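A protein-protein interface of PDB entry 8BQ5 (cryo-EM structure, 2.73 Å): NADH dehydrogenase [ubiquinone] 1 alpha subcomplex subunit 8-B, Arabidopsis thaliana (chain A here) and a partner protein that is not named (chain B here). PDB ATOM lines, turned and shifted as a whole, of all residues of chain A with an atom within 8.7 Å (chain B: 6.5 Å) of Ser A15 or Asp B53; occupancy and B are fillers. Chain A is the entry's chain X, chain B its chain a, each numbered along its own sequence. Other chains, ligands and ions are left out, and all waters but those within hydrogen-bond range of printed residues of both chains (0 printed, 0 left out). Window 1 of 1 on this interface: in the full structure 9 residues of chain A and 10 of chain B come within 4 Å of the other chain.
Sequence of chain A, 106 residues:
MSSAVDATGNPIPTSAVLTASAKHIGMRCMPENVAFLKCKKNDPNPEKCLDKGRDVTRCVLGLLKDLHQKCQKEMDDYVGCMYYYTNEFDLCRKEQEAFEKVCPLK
O of Pro A13 sits at hydrogen-bond distance from NH2 of Arg B52, 2.8 Å away. The side-chain carboxylate (OD1) of Asp B53 sits at hydrogen-bond distance from the side-chain hydroxyl (OG) of Ser A15. The backbone carbonyl oxygen (O) of Tyr A83 sits at hydrogen-bond distance from the guanidinium group (NH1) of Arg B36 (3.2 Å).
Printed residues of chain B that touch a printed residue of chain A: Arg B36, Met B49, Arg B52, Asp B53, Val B56 and Val B57. Of the 18 printed residues of chain A, 7 touch a printed residue of chain B.
Of chain B, only Met B49, Arg B52 and Asp B53 come within 4 Å of Ser A15. Printed residues of chain B within 4 Å of Thr A86: Arg B36 (3.9 Å). Of the printed residues of chain A, Arg B36 touches Tyr A83 (3.2 Å) and Thr A86 (3.9 Å). Asp B53 touches just these residues of chain A: Thr A14 (3.4 Å) and Ser A15 (2.9 Å). Val B56 touches one residue of chain A. Of the printed residues of chain A, Val B57 touches Thr A14. The nearest printed residue of chain B that does not touch Pro A13 is Val B56 (4.05 Å).
Ile A12 touches Val B56. Arg B52 touches Thr A14. OD1 of Asp B53 touches CB of Thr A14, 3.4 Å away. Thr A14 touches Val B57 (CG2 to CG2, 3.9 Å). Met B49 touches Ser A15. N of Ser A15 touches NH1 of Arg B52, 3.6 Å away. NH2 of Arg B52 touches CD1 of Leu A18, 3.9 Å away. Thr A86 touches Arg B36 (OG1 to NH1, 3.9 Å).
The side-chain carboxylate of Glu B50 is in salt-bridge range of the guanidinium group of Arg B36, at 3.5 Å. The guanidinium group of Arg B52 lies within salt-bridge range of the side-chain carboxylate of Asp B53. The side-chain hydroxyl of Thr A19 is in hydrogen-bond range of the backbone carbonyl oxygen of Ser A15, 2.5 Å away.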
ATOM      1  N   ILE A  12      -3.801   8.675  10.989  1.00  0.00           N
ATOM      2  CA  ILE A  12      -3.903   9.681   9.937  1.00  0.00           C
ATOM      3  C   ILE A  12      -3.729  11.049  10.586  1.00  0.00           C
ATOM      4  O   ILE A  12      -4.508  11.411  11.480  1.00  0.00           O
ATOM      5  CB  ILE A  12      -5.242   9.583   9.189  1.00  0.00           C
ATOM      6  CG1 ILE A  12      -5.566   8.123   8.866  1.00  0.00           C
ATOM      7  CG2 ILE A  12      -5.210  10.419   7.920  1.00  0.00           C
ATOM      8  CD1 ILE A  12      -4.615   7.496   7.877  1.00  0.00           C
ATOM      9  N   PRO A  13      -2.738  11.837  10.176  1.00  0.00           N
ATOM     10  CA  PRO A  13      -2.465  13.128  10.833  1.00  0.00           C
ATOM     11  C   PRO A  13      -3.504  14.193  10.494  1.00  0.00           C
ATOM     12  O   PRO A  13      -3.203  15.235   9.906  1.00  0.00           O
ATOM     13  CB  PRO A  13      -1.071  13.473  10.295  1.00  0.00           C
ATOM     14  CG  PRO A  13      -1.054  12.844   8.949  1.00  0.00           C
ATOM     15  CD  PRO A  13      -1.712  11.515   9.171  1.00  0.00           C
ATOM     16  N   THR A  14      -4.752  13.932  10.872  1.00  0.00           N
ATOM     17  CA  THR A  14      -5.811  14.913  10.701  1.00  0.00           C
ATOM     18  C   THR A  14      -5.628  16.052  11.702  1.00  0.00           C
ATOM     19  O   THR A  14      -4.836  15.970  12.644  1.00  0.00           O
ATOM     20  CB  THR A  14      -7.179  14.258  10.866  1.00  0.00           C
ATOM     21  OG1 THR A  14      -7.262  13.645  12.158  1.00  0.00           O
ATOM     22  CG2 THR A  14      -7.401  13.204   9.793  1.00  0.00           C
ATOM     23  N   SER A  15      -6.385  17.133  11.495  1.00  0.00           N
ATOM     24  CA  SER A  15      -6.250  18.304  12.356  1.00  0.00           C
ATOM     25  C   SER A  15      -6.604  17.974  13.801  1.00  0.00           C
ATOM     26  O   SER A  15      -6.016  18.533  14.733  1.00  0.00           O
ATOM     27  CB  SER A  15      -7.119  19.449  11.835  1.00  0.00           C
ATOM     28  OG  SER A  15      -8.492  19.101  11.840  1.00  0.00           O
ATOM     29  N   ALA A  16      -7.556  17.063  14.006  1.00  0.00           N
ATOM     30  CA  ALA A  16      -7.891  16.644  15.363  1.00  0.00           C
ATOM     31  C   ALA A  16      -6.687  16.014  16.053  1.00  0.00           C
ATOM     32  O   ALA A  16      -6.361  16.357  17.193  1.00  0.00           O
ATOM     33  CB  ALA A  16      -9.069  15.671  15.336  1.00  0.00           C
ATOM     34  N   VAL A  17      -5.994  15.108  15.360  1.00  0.00           N
ATOM     35  CA  VAL A  17      -4.856  14.412  15.960  1.00  0.00           C
ATOM     36  C   VAL A  17      -3.724  15.391  16.256  1.00  0.00           C
ATOM     37  O   VAL A  17      -3.146  15.387  17.351  1.00  0.00           O
ATOM     38  CB  VAL A  17      -4.390  13.267  15.042  1.00  0.00           C
ATOM     39  CG1 VAL A  17      -3.019  12.763  15.465  1.00  0.00           C
ATOM     40  CG2 VAL A  17      -5.405  12.138  15.052  1.00  0.00           C
ATOM     41  N   LEU A  18      -3.392  16.245  15.284  1.00  0.00           N
ATOM     42  CA  LEU A  18      -2.299  17.192  15.478  1.00  0.00           C
ATOM     43  C   LEU A  18      -2.614  18.192  16.582  1.00  0.00           C
ATOM     44  O   LEU A  18      -1.748  18.514  17.399  1.00  0.00           O
ATOM     45  CB  LEU A  18      -1.985  17.920  14.170  1.00  0.00           C
ATOM     46  CG  LEU A  18      -1.435  17.064  13.028  1.00  0.00           C
ATOM     47  CD1 LEU A  18      -1.361  17.870  11.742  1.00  0.00           C
ATOM     48  CD2 LEU A  18      -0.070  16.513  13.397  1.00  0.00           C
ATOM     49  N   THR A  19      -3.849  18.694  16.626  1.00  0.00           N
ATOM     50  CA  THR A  19      -4.216  19.636  17.678  1.00  0.00           C
ATOM     51  C   THR A  19      -4.226  18.961  19.044  1.00  0.00           C
ATOM     52  O   THR A  19      -3.837  19.569  20.047  1.00  0.00           O
ATOM     53  CB  THR A  19      -5.577  20.262  17.375  1.00  0.00           C
ATOM     54  OG1 THR A  19      -5.639  20.617  15.988  1.00  0.00           O
ATOM     55  CG2 THR A  19      -5.784  21.508  18.218  1.00  0.00           C
ATOM     56  N   ALA A  20      -4.667  17.702  19.104  1.00  0.00           N
ATOM     57  CA  ALA A  20      -4.631  16.959  20.357  1.00  0.00           C
ATOM     58  C   ALA A  20      -3.206  16.749  20.842  1.00  0.00           C
ATOM     59  O   ALA A  20      -2.942  16.826  22.047  1.00  0.00           O
ATOM     60  CB  ALA A  20      -5.333  15.613  20.187  1.00  0.00           C
ATOM     61  N   SER A  21      -2.280  16.480  19.925  1.00  0.00           N
ATOM     62  CA  SER A  21      -0.894  16.194  20.266  1.00  0.00           C
ATOM     63  C   SER A  21      -0.003  17.428  20.247  1.00  0.00           C
ATOM     64  O   SER A  21       1.210  17.289  20.427  1.00  0.00           O
ATOM     65  CB  SER A  21      -0.323  15.153  19.298  1.00  0.00           C
ATOM     66  OG  SER A  21      -1.000  13.916  19.420  1.00  0.00           O
ATOM     67  N   ALA A  22      -0.576  18.614  20.016  1.00  0.00           N
ATOM     68  CA  ALA A  22       0.218  19.825  19.826  1.00  0.00           C
ATOM     69  C   ALA A  22       1.178  20.087  20.979  1.00  0.00           C
ATOM     70  O   ALA A  22       2.302  20.544  20.756  1.00  0.00           O
ATOM     71  CB  ALA A  22      -0.710  21.022  19.620  1.00  0.00           C
ATOM     72  N   ILE A  25       4.044  17.734  20.665  1.00  0.00           N
ATOM     73  CA  ILE A  25       4.831  18.133  19.472  1.00  0.00           C
ATOM     74  C   ILE A  25       5.714  19.316  19.874  1.00  0.00           C
ATOM     75  O   ILE A  25       6.911  19.279  19.576  1.00  0.00           O
ATOM     76  CB  ILE A  25       3.902  18.443  18.284  1.00  0.00           C
ATOM     77  CG1 ILE A  25       3.112  17.201  17.861  1.00  0.00           C
ATOM     78  CG2 ILE A  25       4.683  19.030  17.119  1.00  0.00           C
ATOM     79  CD1 ILE A  25       2.113  17.441  16.756  1.00  0.00           C
ATOM     80  N   VAL A  79      -8.721  12.461  20.967  1.00  0.00           N
ATOM     81  CA  VAL A  79      -8.833  12.849  19.533  1.00  0.00           C
ATOM     82  C   VAL A  79     -10.315  12.830  19.140  1.00  0.00           C
ATOM     83  O   VAL A  79     -10.730  13.718  18.382  1.00  0.00           O
ATOM     84  CB  VAL A  79      -7.958  11.958  18.625  1.00  0.00           C
ATOM     85  CG1 VAL A  79      -8.338  12.080  17.159  1.00  0.00           C
ATOM     86  CG2 VAL A  79      -6.477  12.226  18.823  1.00  0.00           C
ATOM     87  N   MET A  82     -11.872  16.002  20.726  1.00  0.00           N
ATOM     88  CA  MET A  82     -11.356  17.190  20.001  1.00  0.00           C
ATOM     89  C   MET A  82     -12.081  17.293  18.660  1.00  0.00           C
ATOM     90  O   MET A  82     -12.519  18.398  18.329  1.00  0.00           O
ATOM     91  CB  MET A  82      -9.846  17.094  19.760  1.00  0.00           C
ATOM     92  CG  MET A  82      -9.019  17.345  21.004  1.00  0.00           C
ATOM     93  SD  MET A  82      -9.187  19.031  21.643  1.00  0.00           S
ATOM     94  CE  MET A  82      -7.820  19.834  20.809  1.00  0.00           C
ATOM     95  N   TYR A  83     -12.231  16.181  17.937  1.00  0.00           N
ATOM     96  CA  TYR A  83     -12.898  16.200  16.609  1.00  0.00           C
ATOM     97  C   TYR A  83     -14.358  16.646  16.758  1.00  0.00           C
ATOM     98  O   TYR A  83     -14.796  17.475  15.953  1.00  0.00           O
ATOM     99  CB  TYR A  83     -12.828  14.831  15.921  1.00  0.00           C
ATOM    100  CG  TYR A  83     -13.770  14.698  14.752  1.00  0.00           C
ATOM    101  CD1 TYR A  83     -13.451  15.235  13.518  1.00  0.00           C
ATOM    102  CD2 TYR A  83     -14.997  14.068  14.886  1.00  0.00           C
ATOM    103  CE1 TYR A  83     -14.318  15.140  12.443  1.00  0.00           C
ATOM    104  CE2 TYR A  83     -15.877  13.967  13.822  1.00  0.00           C
ATOM    105  CZ  TYR A  83     -15.536  14.504  12.595  1.00  0.00           C
ATOM    106  OH  TYR A  83     -16.395  14.405  11.540  1.00  0.00           O
ATOM    107  N   THR A  86     -14.438  20.317  17.279  1.00  0.00           N
ATOM    108  CA  THR A  86     -13.587  21.097  16.340  1.00  0.00           C
ATOM    109  C   THR A  86     -12.381  21.675  17.087  1.00  0.00           C
ATOM    110  O   THR A  86     -12.201  22.903  17.026  1.00  0.00           O
ATOM    111  CB  THR A  86     -14.421  22.124  15.559  1.00  0.00           C
ATOM    112  OG1 THR A  86     -15.676  21.542  15.209  1.00  0.00           O
ATOM    113  CG2 THR A  86     -13.735  22.599  14.295  1.00  0.00           C
ATOM    114  N   ASN A  87     -11.636  20.841  17.824  1.00  0.00           N
ATOM    115  CA  ASN A  87     -10.370  21.267  18.484  1.00  0.00           C
ATOM    116  C   ASN A  87     -10.573  22.351  19.551  1.00  0.00           C
ATOM    117  O   ASN A  87      -9.617  23.120  19.765  1.00  0.00           O
ATOM    118  CB  ASN A  87      -9.342  21.707  17.434  1.00  0.00           C
ATOM    119  CG  ASN A  87      -9.190  20.720  16.296  1.00  0.00           C
ATOM    120  OD1 ASN A  87      -9.170  19.512  16.511  1.00  0.00           O
ATOM    121  ND2 ASN A  87      -9.082  21.229  15.080  1.00  0.00           N
ATOM    122  N   PHE A  89     -10.237  23.241  23.160  1.00  0.00           N
ATOM    123  CA  PHE A  89      -9.620  22.610  24.325  1.00  0.00           C
ATOM    124  C   PHE A  89     -10.544  22.628  25.539  1.00  0.00           C
ATOM    125  O   PHE A  89     -10.520  21.702  26.357  1.00  0.00           O
ATOM    126  CB  PHE A  89      -8.293  23.290  24.665  1.00  0.00           C
ATOM    127  CG  PHE A  89      -7.226  23.101  23.626  1.00  0.00           C
ATOM    128  CD1 PHE A  89      -6.397  21.993  23.663  1.00  0.00           C
ATOM    129  CD2 PHE A  89      -7.035  24.040  22.628  1.00  0.00           C
ATOM    130  CE1 PHE A  89      -5.411  21.818  22.718  1.00  0.00           C
ATOM    131  CE2 PHE A  89      -6.051  23.868  21.680  1.00  0.00           C
ATOM    132  CZ  PHE A  89      -5.243  22.751  21.724  1.00  0.00           C
ATOM    133  N   ARG B  36     -20.938  16.748  13.251  1.00  0.00           N
ATOM    134  CA  ARG B  36     -20.515  17.304  14.526  1.00  0.00           C
ATOM    135  C   ARG B  36     -21.244  18.620  14.749  1.00  0.00           C
ATOM    136  O   ARG B  36     -21.699  19.253  13.790  1.00  0.00           O
ATOM    137  CB  ARG B  36     -18.995  17.519  14.575  1.00  0.00           C
ATOM    138  CG  ARG B  36     -18.383  18.107  13.315  1.00  0.00           C
ATOM    139  CD  ARG B  36     -16.870  18.202  13.447  1.00  0.00           C
ATOM    140  NE  ARG B  36     -16.230  18.664  12.222  1.00  0.00           N
ATOM    141  CZ  ARG B  36     -14.928  18.881  12.093  1.00  0.00           C
ATOM    142  NH1 ARG B  36     -14.093  18.694  13.101  1.00  0.00           N
ATOM    143  NH2 ARG B  36     -14.453  19.297  10.923  1.00  0.00           N
ATOM    144  N   ALA B  48      -8.992  26.352   6.672  1.00  0.00           N
ATOM    145  CA  ALA B  48      -7.802  25.724   6.048  1.00  0.00           C
ATOM    146  C   ALA B  48      -7.649  24.283   6.546  1.00  0.00           C
ATOM    147  O   ALA B  48      -7.384  23.407   5.711  1.00  0.00           O
ATOM    148  CB  ALA B  48      -6.579  26.548   6.355  1.00  0.00           C
ATOM    149  N   MET B  49      -7.866  24.045   7.837  1.00  0.00           N
ATOM    150  CA  MET B  49      -7.756  22.683   8.419  1.00  0.00           C
ATOM    151  C   MET B  49      -8.777  21.753   7.764  1.00  0.00           C
ATOM    152  O   MET B  49      -8.362  20.701   7.296  1.00  0.00           O
ATOM    153  CB  MET B  49      -8.003  22.721   9.928  1.00  0.00           C
ATOM    154  CG  MET B  49      -6.848  23.267  10.733  1.00  0.00           C
ATOM    155  SD  MET B  49      -5.241  22.748  10.109  1.00  0.00           S
ATOM    156  CE  MET B  49      -4.632  24.302   9.464  1.00  0.00           C
ATOM    157  N   GLU B  50     -10.051  22.146   7.733  1.00  0.00           N
ATOM    158  CA  GLU B  50     -11.135  21.311   7.154  1.00  0.00           C
ATOM    159  C   GLU B  50     -10.817  20.915   5.708  1.00  0.00           C
ATOM    160  O   GLU B  50     -10.976  19.727   5.381  1.00  0.00           O
ATOM    161  CB  GLU B  50     -12.440  22.095   7.195  1.00  0.00           C
ATOM    162  CG  GLU B  50     -13.222  21.908   8.482  1.00  0.00           C
ATOM    163  CD  GLU B  50     -14.645  22.440   8.441  1.00  0.00           C
ATOM    164  OE1 GLU B  50     -15.349  22.309   9.461  1.00  0.00           O
ATOM    165  OE2 GLU B  50     -15.047  22.988   7.392  1.00  0.00           O
ATOM    166  N   ARG B  51     -10.410  21.869   4.880  1.00  0.00           N
ATOM    167  CA  ARG B  51     -10.127  21.587   3.449  1.00  0.00           C
ATOM    168  C   ARG B  51      -8.947  20.614   3.342  1.00  0.00           C
ATOM    169  O   ARG B  51      -9.053  19.659   2.565  1.00  0.00           O
ATOM    170  CB  ARG B  51      -9.902  22.911   2.707  1.00  0.00           C
ATOM    171  CG  ARG B  51     -11.100  23.843   2.789  1.00  0.00           C
ATOM    172  CD  ARG B  51     -11.004  25.142   2.010  1.00  0.00           C
ATOM    173  NE  ARG B  51     -12.287  25.831   2.082  1.00  0.00           N
ATOM    174  CZ  ARG B  51     -12.565  27.012   1.539  1.00  0.00           C
ATOM    175  NH1 ARG B  51     -11.643  27.673   0.861  1.00  0.00           N
ATOM    176  NH2 ARG B  51     -13.771  27.531   1.683  1.00  0.00           N
ATOM    177  N   ARG B  52      -7.879  20.851   4.103  1.00  0.00           N
ATOM    178  CA  ARG B  52      -6.681  19.969   4.087  1.00  0.00           C
ATOM    179  C   ARG B  52      -7.061  18.590   4.636  1.00  0.00           C
ATOM    180  O   ARG B  52      -6.698  17.602   3.994  1.00  0.00           O
ATOM    181  CB  ARG B  52      -5.557  20.633   4.881  1.00  0.00           C
ATOM    182  CG  ARG B  52      -4.375  19.729   5.182  1.00  0.00           C
ATOM    183  CD  ARG B  52      -4.146  19.608   6.669  1.00  0.00           C
ATOM    184  NE  ARG B  52      -3.069  18.666   6.920  1.00  0.00           N
ATOM    185  CZ  ARG B  52      -3.053  17.791   7.915  1.00  0.00           C
ATOM    186  NH1 ARG B  52      -4.065  17.727   8.764  1.00  0.00           N
ATOM    187  NH2 ARG B  52      -2.024  16.975   8.052  1.00  0.00           N
ATOM    188  N   ASP B  53      -7.794  18.530   5.749  1.00  0.00           N
ATOM    189  CA  ASP B  53      -8.275  17.240   6.310  1.00  0.00           C
ATOM    190  C   ASP B  53      -9.058  16.455   5.262  1.00  0.00           C
ATOM    191  O   ASP B  53      -8.837  15.257   5.184  1.00  0.00           O
ATOM    192  CB  ASP B  53      -9.146  17.437   7.547  1.00  0.00           C
ATOM    193  CG  ASP B  53      -8.344  17.496   8.828  1.00  0.00           C
ATOM    194  OD1 ASP B  53      -8.873  17.049   9.860  1.00  0.00           O
ATOM    195  OD2 ASP B  53      -7.199  17.988   8.780  1.00  0.00           O
ATOM    196  N   LYS B  54      -9.926  17.113   4.490  1.00  0.00           N
ATOM    197  CA  LYS B  54     -10.665  16.418   3.404  1.00  0.00           C
ATOM    198  C   LYS B  54      -9.663  15.641   2.535  1.00  0.00           C
ATOM    199  O   LYS B  54      -9.851  14.431   2.406  1.00  0.00           O
ATOM    200  CB  LYS B  54     -11.498  17.420   2.601  1.00  0.00           C
ATOM    201  CG  LYS B  54     -12.651  18.059   3.360  1.00  0.00           C
ATOM    202  CD  LYS B  54     -13.423  19.056   2.529  1.00  0.00           C
ATOM    203  CE  LYS B  54     -14.585  19.676   3.274  1.00  0.00           C
ATOM    204  NZ  LYS B  54     -15.308  20.666   2.442  1.00  0.00           N
ATOM    205  N   LYS B  55      -8.645  16.306   1.973  1.00  0.00           N
ATOM    206  CA  LYS B  55      -7.589  15.576   1.214  1.00  0.00           C
ATOM    207  C   LYS B  55      -6.934  14.518   2.111  1.00  0.00           C
ATOM    208  O   LYS B  55      -6.901  13.354   1.703  1.00  0.00           O
ATOM    209  CB  LYS B  55      -6.480  16.514   0.737  1.00  0.00           C
ATOM    210  CG  LYS B  55      -6.910  17.927   0.370  1.00  0.00           C
ATOM    211  CD  LYS B  55      -5.733  18.864   0.211  1.00  0.00           C
ATOM    212  CE  LYS B  55      -6.133  20.319   0.108  1.00  0.00           C
ATOM    213  NZ  LYS B  55      -5.286  21.184   0.963  1.00  0.00           N
ATOM    214  N   VAL B  56      -6.474  14.901   3.306  1.00  0.00           N
ATOM    215  CA  VAL B  56      -5.742  13.975   4.164  1.00  0.00           C
ATOM    216  C   VAL B  56      -6.559  12.722   4.460  1.00  0.00           C
ATOM    217  O   VAL B  56      -5.992  11.637   4.634  1.00  0.00           O
ATOM    218  CB  VAL B  56      -5.309  14.709   5.452  1.00  0.00           C
ATOM    219  CG1 VAL B  56      -4.851  13.736   6.526  1.00  0.00           C
ATOM    220  CG2 VAL B  56      -4.203  15.706   5.137  1.00  0.00           C
ATOM    221  N   VAL B  57      -7.886  12.835   4.482  1.00  0.00           N
ATOM    222  CA  VAL B  57      -8.752  11.687   4.718  1.00  0.00           C
ATOM    223  C   VAL B  57      -9.021  10.948   3.412  1.00  0.00           C
ATOM    224  O   VAL B  57      -8.816   9.732   3.327  1.00  0.00           O
ATOM    225  CB  VAL B  57     -10.071  12.115   5.386  1.00  0.00           C
ATOM    226  CG1 VAL B  57     -11.036  10.943   5.446  1.00  0.00           C
ATOM    227  CG2 VAL B  57      -9.809  12.655   6.784  1.00  0.00           C
ATOM    228  N   GLU B  58      -9.481  11.670   2.384  1.00  0.00           N
ATOM    229  CA  GLU B  58      -9.964  10.999   1.179  1.00  0.00           C
ATOM    230  C   GLU B  58      -8.829  10.351   0.393  1.00  0.00           C
ATOM    231  O   GLU B  58      -9.024   9.306  -0.239  1.00  0.00           O
ATOM    232  CB  GLU B  58     -10.735  11.986   0.303  1.00  0.00           C
ATOM    233  CG  GLU B  58     -11.291  11.373  -0.972  1.00  0.00           C
ATOM    234  CD  GLU B  58     -12.408  12.193  -1.577  1.00  0.00           C
ATOM    235  OE1 GLU B  58     -12.422  13.425  -1.381  1.00  0.00           O
ATOM    236  OE2 GLU B  58     -13.271  11.602  -2.260  1.00  0.00           O
